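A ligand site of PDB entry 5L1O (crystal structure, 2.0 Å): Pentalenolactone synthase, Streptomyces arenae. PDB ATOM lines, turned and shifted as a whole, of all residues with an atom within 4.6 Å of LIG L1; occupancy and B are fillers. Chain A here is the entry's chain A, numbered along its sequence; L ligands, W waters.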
ATOM      1  N   MET A  84       7.046 -23.649  -6.760  1.00  0.00           N
ATOM      2  CA  MET A  84       6.092 -24.606  -7.322  1.00  0.00           C
ATOM      3  C   MET A  84       6.421 -24.962  -8.763  1.00  0.00           C
ATOM      4  O   MET A  84       5.581 -25.570  -9.441  1.00  0.00           O
ATOM      5  CB  MET A  84       4.667 -24.057  -7.206  1.00  0.00           C
ATOM      6  CG  MET A  84       4.179 -24.019  -5.732  1.00  0.00           C
ATOM      7  SD  MET A  84       2.654 -23.072  -5.471  1.00  0.00           S
ATOM      8  CE  MET A  84       1.434 -24.212  -6.129  1.00  0.00           C
ATOM      9  N   HIS A  96       7.563 -29.651 -13.038  1.00  0.00           N
ATOM     10  CA  HIS A  96       6.511 -29.923 -12.056  1.00  0.00           C
ATOM     11  C   HIS A  96       6.292 -31.413 -11.898  1.00  0.00           C
ATOM     12  O   HIS A  96       6.061 -31.888 -10.780  1.00  0.00           O
ATOM     13  CB  HIS A  96       5.201 -29.241 -12.441  1.00  0.00           C
ATOM     14  CG  HIS A  96       4.106 -29.498 -11.457  1.00  0.00           C
ATOM     15  ND1 HIS A  96       2.919 -30.115 -11.800  1.00  0.00           N
ATOM     16  CD2 HIS A  96       4.020 -29.238 -10.126  1.00  0.00           C
ATOM     17  CE1 HIS A  96       2.155 -30.214 -10.721  1.00  0.00           C
ATOM     18  NE2 HIS A  96       2.803 -29.699  -9.698  1.00  0.00           N
ATOM     19  N   MET A  99       8.986 -32.494  -9.633  1.00  0.00           N
ATOM     20  CA  MET A  99       8.742 -32.023  -8.278  1.00  0.00           C
ATOM     21  C   MET A  99       7.835 -32.984  -7.516  1.00  0.00           C
ATOM     22  O   MET A  99       8.160 -33.423  -6.408  1.00  0.00           O
ATOM     23  CB  MET A  99       8.148 -30.605  -8.295  1.00  0.00           C
ATOM     24  CG  MET A  99       7.777 -30.125  -6.913  1.00  0.00           C
ATOM     25  SD  MET A  99       7.027 -28.481  -6.934  1.00  0.00           S
ATOM     26  CE  MET A  99       7.084 -28.126  -5.162  1.00  0.00           C
ATOM     27  N   ARG A 100       6.692 -33.347  -8.116  1.00  0.00           N
ATOM     28  CA  ARG A 100       5.765 -34.246  -7.433  1.00  0.00           C
ATOM     29  C   ARG A 100       6.351 -35.645  -7.295  1.00  0.00           C
ATOM     30  O   ARG A 100       6.173 -36.283  -6.248  1.00  0.00           O
ATOM     31  CB  ARG A 100       4.424 -34.265  -8.173  1.00  0.00           C
ATOM     32  CG  ARG A 100       3.706 -32.918  -8.087  1.00  0.00           C
ATOM     33  CD  ARG A 100       2.229 -32.999  -8.483  1.00  0.00           C
ATOM     34  NE  ARG A 100       1.416 -33.861  -7.620  1.00  0.00           N
ATOM     35  CZ  ARG A 100       0.719 -33.449  -6.558  1.00  0.00           C
ATOM     36  NH1 ARG A 100       0.748 -32.169  -6.176  1.00  0.00           N
ATOM     37  NH2 ARG A 100      -0.011 -34.311  -5.870  1.00  0.00           N
ATOM     38  N   LEU A 103       8.719 -35.522  -4.252  1.00  0.00           N
ATOM     39  CA  LEU A 103       8.167 -35.198  -2.940  1.00  0.00           C
ATOM     40  C   LEU A 103       7.180 -36.240  -2.418  1.00  0.00           C
ATOM     41  O   LEU A 103       7.163 -36.526  -1.211  1.00  0.00           O
ATOM     42  CB  LEU A 103       7.481 -33.816  -2.990  1.00  0.00           C
ATOM     43  CG  LEU A 103       8.434 -32.614  -3.040  1.00  0.00           C
ATOM     44  CD1 LEU A 103       7.648 -31.291  -3.034  1.00  0.00           C
ATOM     45  CD2 LEU A 103       9.403 -32.653  -1.869  1.00  0.00           C
ATOM     46  N   PHE A 107       6.471 -38.829   1.977  1.00  0.00           N
ATOM     47  CA  PHE A 107       5.361 -38.880   2.916  1.00  0.00           C
ATOM     48  C   PHE A 107       4.753 -40.277   2.895  1.00  0.00           C
ATOM     49  O   PHE A 107       3.549 -40.447   2.700  1.00  0.00           O
ATOM     50  CB  PHE A 107       4.339 -37.796   2.579  1.00  0.00           C
ATOM     51  CG  PHE A 107       4.893 -36.380   2.681  1.00  0.00           C
ATOM     52  CD1 PHE A 107       5.512 -35.787   1.586  1.00  0.00           C
ATOM     53  CD2 PHE A 107       4.805 -35.667   3.877  1.00  0.00           C
ATOM     54  CE1 PHE A 107       6.047 -34.503   1.680  1.00  0.00           C
ATOM     55  CE2 PHE A 107       5.330 -34.384   3.970  1.00  0.00           C
ATOM     56  CZ  PHE A 107       5.961 -33.797   2.869  1.00  0.00           C
ATOM     57  N   LEU A 155      10.539 -33.517   9.850  1.00  0.00           N
ATOM     58  CA  LEU A 155      10.710 -33.791   8.429  1.00  0.00           C
ATOM     59  C   LEU A 155      12.112 -33.422   7.942  1.00  0.00           C
ATOM     60  O   LEU A 155      12.702 -34.142   7.141  1.00  0.00           O
ATOM     61  CB  LEU A 155       9.667 -33.025   7.601  1.00  0.00           C
ATOM     62  CG  LEU A 155       8.199 -33.435   7.701  1.00  0.00           C
ATOM     63  CD1 LEU A 155       7.370 -32.428   6.900  1.00  0.00           C
ATOM     64  CD2 LEU A 155       7.996 -34.854   7.165  1.00  0.00           C
ATOM     65  N   PHE A 235       5.987 -24.171   2.715  1.00  0.00           N
ATOM     66  CA  PHE A 235       4.583 -24.589   2.630  1.00  0.00           C
ATOM     67  C   PHE A 235       4.157 -25.531   3.758  1.00  0.00           C
ATOM     68  O   PHE A 235       2.962 -25.750   3.961  1.00  0.00           O
ATOM     69  CB  PHE A 235       4.280 -25.289   1.286  1.00  0.00           C
ATOM     70  CG  PHE A 235       4.612 -24.446   0.058  1.00  0.00           C
ATOM     71  CD1 PHE A 235       4.961 -25.068  -1.139  1.00  0.00           C
ATOM     72  CD2 PHE A 235       4.575 -23.057   0.108  1.00  0.00           C
ATOM     73  CE1 PHE A 235       5.265 -24.309  -2.281  1.00  0.00           C
ATOM     74  CE2 PHE A 235       4.874 -22.277  -1.027  1.00  0.00           C
ATOM     75  CZ  PHE A 235       5.224 -22.907  -2.217  1.00  0.00           C
ATOM     76  N   GLY A 236       5.105 -26.082   4.510  1.00  0.00           N
ATOM     77  CA  GLY A 236       4.833 -27.183   5.423  1.00  0.00           C
ATOM     78  C   GLY A 236       4.449 -26.864   6.855  1.00  0.00           C
ATOM     79  O   GLY A 236       4.175 -27.812   7.595  1.00  0.00           O
ATOM     80  N   THR A 239       0.422 -22.768   6.861  1.00  0.00           N
ATOM     81  CA  THR A 239      -1.004 -22.950   6.589  1.00  0.00           C
ATOM     82  C   THR A 239      -1.656 -23.869   7.619  1.00  0.00           C
ATOM     83  O   THR A 239      -2.836 -23.693   7.945  1.00  0.00           O
ATOM     84  CB  THR A 239      -1.248 -23.504   5.165  1.00  0.00           C
ATOM     85  OG1 THR A 239      -0.575 -24.756   4.991  1.00  0.00           O
ATOM     86  CG2 THR A 239      -0.797 -22.501   4.085  1.00  0.00           C
ATOM     87  N   THR A 240      -0.917 -24.857   8.139  1.00  0.00           N
ATOM     88  CA  THR A 240      -1.442 -25.706   9.208  1.00  0.00           C
ATOM     89  C   THR A 240      -1.687 -24.904  10.488  1.00  0.00           C
ATOM     90  O   THR A 240      -2.714 -25.089  11.170  1.00  0.00           O
ATOM     91  CB  THR A 240      -0.482 -26.863   9.470  1.00  0.00           C
ATOM     92  OG1 THR A 240      -0.174 -27.512   8.232  1.00  0.00           O
ATOM     93  CG2 THR A 240      -1.088 -27.888  10.431  1.00  0.00           C
ATOM     94  N   ARG A 243      -4.902 -23.168  10.171  1.00  0.00           N
ATOM     95  CA  ARG A 243      -6.071 -24.039  10.313  1.00  0.00           C
ATOM     96  C   ARG A 243      -6.335 -24.446  11.763  1.00  0.00           C
ATOM     97  O   ARG A 243      -7.490 -24.674  12.143  1.00  0.00           O
ATOM     98  CB  ARG A 243      -5.939 -25.294   9.431  1.00  0.00           C
ATOM     99  CG  ARG A 243      -5.863 -25.001   7.910  1.00  0.00           C
ATOM    100  CD  ARG A 243      -6.782 -23.844   7.560  1.00  0.00           C
ATOM    101  NE  ARG A 243      -6.840 -23.481   6.133  1.00  0.00           N
ATOM    102  CZ  ARG A 243      -5.953 -22.711   5.518  1.00  0.00           C
ATOM    103  NH1 ARG A 243      -4.891 -22.269   6.176  1.00  0.00           N
ATOM    104  NH2 ARG A 243      -6.116 -22.388   4.241  1.00  0.00           N
ATOM    105  N   LEU A 276     -11.675 -27.694   7.726  1.00  0.00           N
ATOM    106  CA  LEU A 276     -11.014 -27.372   6.463  1.00  0.00           C
ATOM    107  C   LEU A 276     -11.993 -26.758   5.474  1.00  0.00           C
ATOM    108  O   LEU A 276     -11.656 -25.821   4.734  1.00  0.00           O
ATOM    109  CB  LEU A 276     -10.369 -28.637   5.885  1.00  0.00           C
ATOM    110  CG  LEU A 276      -9.180 -29.243   6.658  1.00  0.00           C
ATOM    111  CD1 LEU A 276      -8.893 -30.666   6.202  1.00  0.00           C
ATOM    112  CD2 LEU A 276      -7.946 -28.368   6.474  1.00  0.00           C
ATOM    113  N   ILE A 289      -7.328 -20.223  -5.725  1.00  0.00           N
ATOM    114  CA  ILE A 289      -6.221 -20.877  -6.418  1.00  0.00           C
ATOM    115  C   ILE A 289      -6.027 -20.175  -7.761  1.00  0.00           C
ATOM    116  O   ILE A 289      -6.950 -20.185  -8.593  1.00  0.00           O
ATOM    117  CB  ILE A 289      -6.466 -22.373  -6.613  1.00  0.00           C
ATOM    118  CG1 ILE A 289      -6.466 -23.094  -5.255  1.00  0.00           C
ATOM    119  CG2 ILE A 289      -5.385 -22.934  -7.541  1.00  0.00           C
ATOM    120  CD1 ILE A 289      -6.626 -24.628  -5.348  1.00  0.00           C
ATOM    121  N   ARG A 291      -4.735 -19.372 -11.610  1.00  0.00           N
ATOM    122  CA  ARG A 291      -4.356 -20.104 -12.822  1.00  0.00           C
ATOM    123  C   ARG A 291      -4.320 -19.157 -14.019  1.00  0.00           C
ATOM    124  O   ARG A 291      -4.844 -18.044 -13.966  1.00  0.00           O
ATOM    125  CB  ARG A 291      -5.322 -21.266 -13.122  1.00  0.00           C
ATOM    126  CG  ARG A 291      -5.336 -22.422 -12.086  1.00  0.00           C
ATOM    127  CD  ARG A 291      -4.037 -23.221 -12.112  1.00  0.00           C
ATOM    128  NE  ARG A 291      -4.064 -24.419 -11.251  1.00  0.00           N
ATOM    129  CZ  ARG A 291      -3.533 -24.498 -10.035  1.00  0.00           C
ATOM    130  NH1 ARG A 291      -2.909 -23.435  -9.495  1.00  0.00           N
ATOM    131  NH2 ARG A 291      -3.609 -25.637  -9.341  1.00  0.00           N
ATOM    132  N   ILE A 314     -11.861 -21.756  -4.062  1.00  0.00           N
ATOM    133  CA  ILE A 314     -12.087 -22.977  -3.290  1.00  0.00           C
ATOM    134  C   ILE A 314     -12.847 -22.678  -1.996  1.00  0.00           C
ATOM    135  O   ILE A 314     -13.674 -23.493  -1.561  1.00  0.00           O
ATOM    136  CB  ILE A 314     -10.757 -23.704  -2.996  1.00  0.00           C
ATOM    137  CG1 ILE A 314      -9.743 -22.798  -2.286  1.00  0.00           C
ATOM    138  CG2 ILE A 314     -10.149 -24.277  -4.281  1.00  0.00           C
ATOM    139  CD1 ILE A 314      -8.408 -23.475  -1.940  1.00  0.00           C
ATOM    140  N   ALA A 342     -10.376 -27.712  -0.007  1.00  0.00           N
ATOM    141  CA  ALA A 342      -9.402 -26.884   0.710  1.00  0.00           C
ATOM    142  C   ALA A 342      -7.952 -27.291   0.466  1.00  0.00           C
ATOM    143  O   ALA A 342      -7.036 -26.486   0.711  1.00  0.00           O
ATOM    144  CB  ALA A 342      -9.671 -26.905   2.216  1.00  0.00           C
ATOM    145  N   PHE A 343      -7.695 -28.518   0.014  1.00  0.00           N
ATOM    146  CA  PHE A 343      -6.370 -28.956  -0.417  1.00  0.00           C
ATOM    147  C   PHE A 343      -6.206 -28.908  -1.935  1.00  0.00           C
ATOM    148  O   PHE A 343      -5.205 -29.410  -2.465  1.00  0.00           O
ATOM    149  CB  PHE A 343      -6.096 -30.395   0.052  1.00  0.00           C
ATOM    150  CG  PHE A 343      -5.927 -30.542   1.557  1.00  0.00           C
ATOM    151  CD1 PHE A 343      -4.940 -29.833   2.235  1.00  0.00           C
ATOM    152  CD2 PHE A 343      -6.731 -31.422   2.285  1.00  0.00           C
ATOM    153  CE1 PHE A 343      -4.776 -29.985   3.619  1.00  0.00           C
ATOM    154  CE2 PHE A 343      -6.564 -31.589   3.667  1.00  0.00           C
ATOM    155  CZ  PHE A 343      -5.579 -30.851   4.332  1.00  0.00           C
ATOM    156  N   GLY A 344      -7.155 -28.315  -2.644  1.00  0.00           N
ATOM    157  CA  GLY A 344      -7.100 -28.357  -4.078  1.00  0.00           C
ATOM    158  C   GLY A 344      -7.621 -29.675  -4.642  1.00  0.00           C
ATOM    159  O   GLY A 344      -8.362 -30.423  -3.995  1.00  0.00           O
ATOM    160  N   ALA A 347      -3.908 -31.812 -10.664  1.00  0.00           N
ATOM    161  CA  ALA A 347      -2.473 -31.971 -10.851  1.00  0.00           C
ATOM    162  C   ALA A 347      -1.663 -31.448  -9.666  1.00  0.00           C
ATOM    163  O   ALA A 347      -0.577 -31.977  -9.388  1.00  0.00           O
ATOM    164  CB  ALA A 347      -2.022 -31.267 -12.126  1.00  0.00           C
ATOM    165  N   ARG A 348      -2.144 -30.417  -8.976  1.00  0.00           N
ATOM    166  CA  ARG A 348      -1.375 -29.819  -7.886  1.00  0.00           C
ATOM    167  C   ARG A 348      -1.978 -30.084  -6.507  1.00  0.00           C
ATOM    168  O   ARG A 348      -1.670 -29.356  -5.555  1.00  0.00           O
ATOM    169  CB  ARG A 348      -1.207 -28.315  -8.143  1.00  0.00           C
ATOM    170  CG  ARG A 348      -0.308 -27.992  -9.355  1.00  0.00           C
ATOM    171  CD  ARG A 348      -0.054 -26.468  -9.508  1.00  0.00           C
ATOM    172  NE  ARG A 348       0.907 -26.188 -10.593  1.00  0.00           N
ATOM    173  CZ  ARG A 348       2.226 -26.157 -10.418  1.00  0.00           C
ATOM    174  NH1 ARG A 348       2.744 -26.395  -9.222  1.00  0.00           N
ATOM    175  NH2 ARG A 348       3.038 -25.886 -11.436  1.00  0.00           N
ATOM    176  N   HIS A 349      -2.833 -31.107  -6.404  1.00  0.00           N
ATOM    177  CA  HIS A 349      -3.418 -31.539  -5.128  1.00  0.00           C
ATOM    178  C   HIS A 349      -2.361 -31.620  -4.033  1.00  0.00           C
ATOM    179  O   HIS A 349      -1.322 -32.257  -4.214  1.00  0.00           O
ATOM    180  CB  HIS A 349      -4.078 -32.913  -5.326  1.00  0.00           C
ATOM    181  CG  HIS A 349      -5.162 -33.240  -4.343  1.00  0.00           C
ATOM    182  ND1 HIS A 349      -5.848 -34.441  -4.389  1.00  0.00           N
ATOM    183  CD2 HIS A 349      -5.676 -32.548  -3.299  1.00  0.00           C
ATOM    184  CE1 HIS A 349      -6.742 -34.474  -3.408  1.00  0.00           C
ATOM    185  NE2 HIS A 349      -6.656 -33.332  -2.739  1.00  0.00           N
ATOM    186  N   CYS A 350      -2.645 -30.973  -2.898  1.00  0.00           N
ATOM    187  CA  CYS A 350      -1.689 -30.782  -1.821  1.00  0.00           C
ATOM    188  C   CYS A 350      -0.914 -32.062  -1.478  1.00  0.00           C
ATOM    189  O   CYS A 350      -1.504 -33.103  -1.186  1.00  0.00           O
ATOM    190  CB  CYS A 350      -2.427 -30.265  -0.574  1.00  0.00           C
ATOM    191  SG  CYS A 350      -1.450 -30.307   0.940  1.00  0.00           S
ATOM    192  N   ILE A 351       0.416 -31.955  -1.483  1.00  0.00           N
ATOM    193  CA  ILE A 351       1.281 -33.098  -1.203  1.00  0.00           C
ATOM    194  C   ILE A 351       1.268 -33.445   0.287  1.00  0.00           C
ATOM    195  O   ILE A 351       1.381 -34.628   0.667  1.00  0.00           O
ATOM    196  CB  ILE A 351       2.705 -32.790  -1.711  1.00  0.00           C
ATOM    197  CG1 ILE A 351       2.722 -32.829  -3.243  1.00  0.00           C
ATOM    198  CG2 ILE A 351       3.723 -33.778  -1.144  1.00  0.00           C
ATOM    199  CD1 ILE A 351       4.085 -32.601  -3.818  1.00  0.00           C
ATOM    200  N   GLY A 352       1.127 -32.457   1.166  1.00  0.00           N
ATOM    201  CA  GLY A 352       1.191 -32.726   2.590  1.00  0.00           C
ATOM    202  C   GLY A 352      -0.134 -33.021   3.267  1.00  0.00           C
ATOM    203  O   GLY A 352      -0.177 -33.097   4.506  1.00  0.00           O
ATOM    204  N   LEU A 355      -0.534 -35.709   6.071  1.00  0.00           N
ATOM    205  CA  LEU A 355       0.151 -35.255   7.274  1.00  0.00           C
ATOM    206  C   LEU A 355      -0.600 -34.116   7.956  1.00  0.00           C
ATOM    207  O   LEU A 355      -0.720 -34.089   9.189  1.00  0.00           O
ATOM    208  CB  LEU A 355       1.572 -34.850   6.912  1.00  0.00           C
ATOM    209  CG  LEU A 355       2.430 -34.239   8.013  1.00  0.00           C
ATOM    210  CD1 LEU A 355       2.586 -35.262   9.152  1.00  0.00           C
ATOM    211  CD2 LEU A 355       3.779 -33.848   7.435  1.00  0.00           C
ATOM    212  N   ALA A 356      -1.102 -33.138   7.187  1.00  0.00           N
ATOM    213  CA  ALA A 356      -1.856 -32.040   7.781  1.00  0.00           C
ATOM    214  C   ALA A 356      -3.096 -32.545   8.525  1.00  0.00           C
ATOM    215  O   ALA A 356      -3.422 -32.047   9.607  1.00  0.00           O
ATOM    216  CB  ALA A 356      -2.266 -31.015   6.711  1.00  0.00           C
ATOM    217  N   LEU A 360      -4.082 -32.016  12.600  1.00  0.00           N
ATOM    218  CA  LEU A 360      -5.332 -31.401  13.025  1.00  0.00           C
ATOM    219  C   LEU A 360      -6.197 -32.385  13.806  1.00  0.00           C
ATOM    220  O   LEU A 360      -6.858 -32.009  14.786  1.00  0.00           O
ATOM    221  CB  LEU A 360      -6.086 -30.856  11.797  1.00  0.00           C
ATOM    222  CG  LEU A 360      -5.455 -29.680  11.023  1.00  0.00           C
ATOM    223  CD1 LEU A 360      -6.254 -29.334   9.747  1.00  0.00           C
ATOM    224  CD2 LEU A 360      -5.322 -28.427  11.908  1.00  0.00           C
HETATM  225  C1  LIG L   1      -0.247 -27.477  -2.495  1.00  0.00           C
HETATM  226  C2  LIG L   1      -3.459 -26.369   0.986  1.00  0.00           C
HETATM  227  C3  LIG L   1      -0.441 -28.246   4.318  1.00  0.00           C
HETATM  228  C4  LIG L   1       2.885 -29.094   0.902  1.00  0.00           C
HETATM  229  C5  LIG L   1      -1.409 -27.066  -1.867  1.00  0.00           C
HETATM  230  C6  LIG L   1      -2.602 -26.534  -2.514  1.00  0.00           C
HETATM  231  C7  LIG L   1      -3.475 -26.241  -1.541  1.00  0.00           C
HETATM  232  C8  LIG L   1      -2.874 -26.560  -0.261  1.00  0.00           C
HETATM  233  C9  LIG L   1      -4.892 -25.629  -1.721  1.00  0.00           C
HETATM  234  C10 LIG L   1      -2.819 -26.380  -4.054  1.00  0.00           C
HETATM  235  C11 LIG L   1      -2.212 -25.082  -4.627  1.00  0.00           C
HETATM  236  C12 LIG L   1      -2.532 -24.952  -6.116  1.00  0.00           C
HETATM  237  O1  LIG L   1      -3.257 -25.801  -6.689  1.00  0.00           O
HETATM  238  O2  LIG L   1      -2.051 -23.973  -6.758  1.00  0.00           O
HETATM  239  C13 LIG L   1      -2.933 -26.749   2.206  1.00  0.00           C
HETATM  240  C14 LIG L   1      -3.565 -26.631   3.509  1.00  0.00           C
HETATM  241  C15 LIG L   1      -2.715 -27.135   4.415  1.00  0.00           C
HETATM  242  C16 LIG L   1      -1.531 -27.634   3.722  1.00  0.00           C
HETATM  243  C17 LIG L   1      -4.950 -25.985   3.754  1.00  0.00           C
HETATM  244  C18 LIG L   1      -2.888 -27.271   5.943  1.00  0.00           C
HETATM  245  C19 LIG L   1      -4.069 -27.499   6.526  1.00  0.00           C
HETATM  246  C20 LIG L   1       0.714 -28.687   3.702  1.00  0.00           C
HETATM  247  C21 LIG L   1       1.796 -29.408   4.330  1.00  0.00           C
HETATM  248  C22 LIG L   1       2.728 -29.642   3.373  1.00  0.00           C
HETATM  249  C23 LIG L   1       2.240 -29.084   2.121  1.00  0.00           C
HETATM  250  C24 LIG L   1       1.797 -29.795   5.835  1.00  0.00           C
HETATM  251  C25 LIG L   1       4.101 -30.360   3.473  1.00  0.00           C
HETATM  252  C26 LIG L   1       4.703 -30.656   4.634  1.00  0.00           C
HETATM  253  C27 LIG L   1       2.341 -28.674  -0.304  1.00  0.00           C
HETATM  254  C28 LIG L   1       3.034 -28.626  -1.566  1.00  0.00           C
HETATM  255  C29 LIG L   1       2.189 -28.192  -2.502  1.00  0.00           C
HETATM  256  C30 LIG L   1       0.905 -27.929  -1.865  1.00  0.00           C
HETATM  257  C31 LIG L   1       4.510 -29.029  -1.778  1.00  0.00           C
HETATM  258  C32 LIG L   1       2.496 -27.964  -3.996  1.00  0.00           C
HETATM  259  C33 LIG L   1       1.812 -29.053  -4.836  1.00  0.00           C
HETATM  260  C34 LIG L   1       2.057 -28.836  -6.310  1.00  0.00           C
HETATM  261  O3  LIG L   1       2.073 -29.838  -7.069  1.00  0.00           O
HETATM  262  O4  LIG L   1       2.256 -27.653  -6.744  1.00  0.00           O
HETATM  263  N1  LIG L   1      -1.613 -27.068  -0.502  1.00  0.00           N
HETATM  264  N2  LIG L   1      -1.708 -27.370   2.384  1.00  0.00           N
HETATM  265  N3  LIG L   1       1.009 -28.506   2.362  1.00  0.00           N
HETATM  266  N4  LIG L   1       1.048 -28.235  -0.525  1.00  0.00           N
HETATM  267 FE1  LIG L   1      -0.425 -28.049   0.892  1.00  0.00          FE
HETATM  268  C1  LG2 L   2      -0.982 -23.847  -0.701  1.00  0.00           C
HETATM  269  C2  LG2 L   2       0.236 -22.965  -1.008  1.00  0.00           C
HETATM  270  C3  LG2 L   2       1.293 -23.777  -1.762  1.00  0.00           C
HETATM  271  C4  LG2 L   2       0.919 -22.420   0.263  1.00  0.00           C
HETATM  272  C5  LG2 L   2      -2.975 -22.671   0.394  1.00  0.00           C
HETATM  273  C6  LG2 L   2      -2.497 -19.362  -0.476  1.00  0.00           C
HETATM  274  C7  LG2 L   2      -4.167 -21.387  -2.622  1.00  0.00           C
HETATM  275  C8  LG2 L   2      -0.386 -21.882  -1.923  1.00  0.00           C
HETATM  276  C9  LG2 L   2      -3.240 -20.853   1.970  1.00  0.00           C
HETATM  277  C10 LG2 L   2      -2.292 -19.731  -2.852  1.00  0.00           C
HETATM  278  C11 LG2 L   2      -2.706 -21.404   0.840  1.00  0.00           C
HETATM  279  C12 LG2 L   2      -2.291 -22.975  -0.845  1.00  0.00           C
HETATM  280  C13 LG2 L   2      -1.846 -20.734  -0.080  1.00  0.00           C
HETATM  281  C14 LG2 L   2      -2.698 -21.031  -2.489  1.00  0.00           C
HETATM  282  C15 LG2 L   2      -1.816 -21.612  -1.347  1.00  0.00           C
HETATM  283  O1  LG2 L   2      -4.099 -21.455   2.643  1.00  0.00           O
HETATM  284  O2  LG2 L   2      -2.129 -19.416  -4.033  1.00  0.00           O
HETATM  285  O3  LG2 L   2      -2.879 -19.730   2.422  1.00  0.00           O
HETATM  286  O4  LG2 L   2      -2.077 -18.876  -1.806  1.00  0.00           O
HETATM  287  O5  LG2 L   2      -3.144 -21.915  -3.528  1.00  0.00           O
HETATM  288  O   HOH W   1       0.702 -25.187   2.601  1.00  0.00           O
HETATM  289  O   HOH W   2      -1.240 -21.524  -5.992  1.00  0.00           O
HETATM  290  O   HOH W   3      -4.748 -28.051  -6.675  1.00  0.00           O
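SG of Cys 350 is bound to FE1 of LIG L1, at 2.5 Å.
A ring nitrogen (NE2) of His 96 is in hydrogen-bond range of an oxygen (O3) of LIG L1, at 2.7 Å.
O4 of LIG L1 lies within salt-bridge range of NH1 of Arg 348, 2.8 Å away.
NH1 of Arg 100 is in salt-bridge range of O3 of LIG L1, 2.8 Å away.
The guanidinium group (NH2) of Arg 291 lies within salt-bridge range of an oxygen (O1) of LIG L1.
An oxygen (O1) of LG2 L2 lies within salt-bridge range of the guanidinium group (NH2) of Arg 243 (2.7 Å).
Met 84 touches LIG L1 (CE to O2, 3.5 Å).
CZ of Phe 107 touches C26 of LIG L1, at 3.8 Å.
Leu 155 touches LIG L1.
Phe 235 touches LIG L1 (O to C20, 3.7 Å).
O of Gly 236 touches C24 of LIG L1, 3.6 Å away.
Thr 239 touches LIG L1 (OG1 to C15, 3.3 Å).
OG1 of Thr 240 touches C18 of LIG L1, at 3.6 Å.
Arg 243 touches LIG L1.
CD2 of Leu 276 touches C19 of LIG L1 (3.97 Å).
CG2 of Ile 289 touches O2 of LIG L1, 3.6 Å away.
O of Ala 342 touches C9 of LIG L1, at 3.4 Å.
C of Phe 343 touches C9 of LIG L1 (3.5 Å).
Gly 344 touches LIG L1 (N to C9, 3.6 Å).
Ile 351 touches LIG L1 (N to N4, 3.9 Å).
Gly 352 touches LIG L1 (CA to C22, 3.5 Å).
Ala 356 touches LIG L1.
Hydrophobic or aromatic side chains within 4 Å of LIG L1: Met 84, His 96, Phe 107, Leu 155, Leu 276, Ile 289, Phe 343 and Ala 356.
21 residues have an atom within 4 Å of LIG L1: Met 84, His 96, Arg 100, Phe 107, Leu 155, Phe 235, Gly 236, Thr 239, Thr 240, Arg 243, Leu 276, Ile 289, Arg 291, Ala 342, Phe 343, Gly 344, Arg 348, Cys 350, Ile 351, Gly 352 and Ala 356.
NE2 of His 96 lies close to NH1 of Arg 348 (3.3 Å).
The guanidinium group of Arg 348 is in hydrogen-bond range of the backbone carbonyl oxygen of Met 84.
The side-chain sulfur (SG) of Cys 350 sits close to the backbone NH (N) of Gly 352, at 3.4 Å.
The guanidinium group (NE) of Arg 100 sits close to the backbone carbonyl oxygen (O) of Ala 347, at 3.3 Å.
NH1 of Arg 100 sits at hydrogen-bond distance from O of His 349 (2.9 Å).
N of Cys 350 sits at hydrogen-bond distance from O of Phe 343.
The backbone carbonyl oxygen of Thr 239 is in hydrogen-bond range of the guanidinium group of Arg 243 (3.1 Å).
Water W2 lies within hydrogen-bond range of O2 of LIG L1 (2.7 Å) and O2 of LG2 L2 (3.0 Å).
Water W1 lies within hydrogen-bond range of the backbone carbonyl oxygen of Phe 235 and the side-chain hydroxyl of Thr 239.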
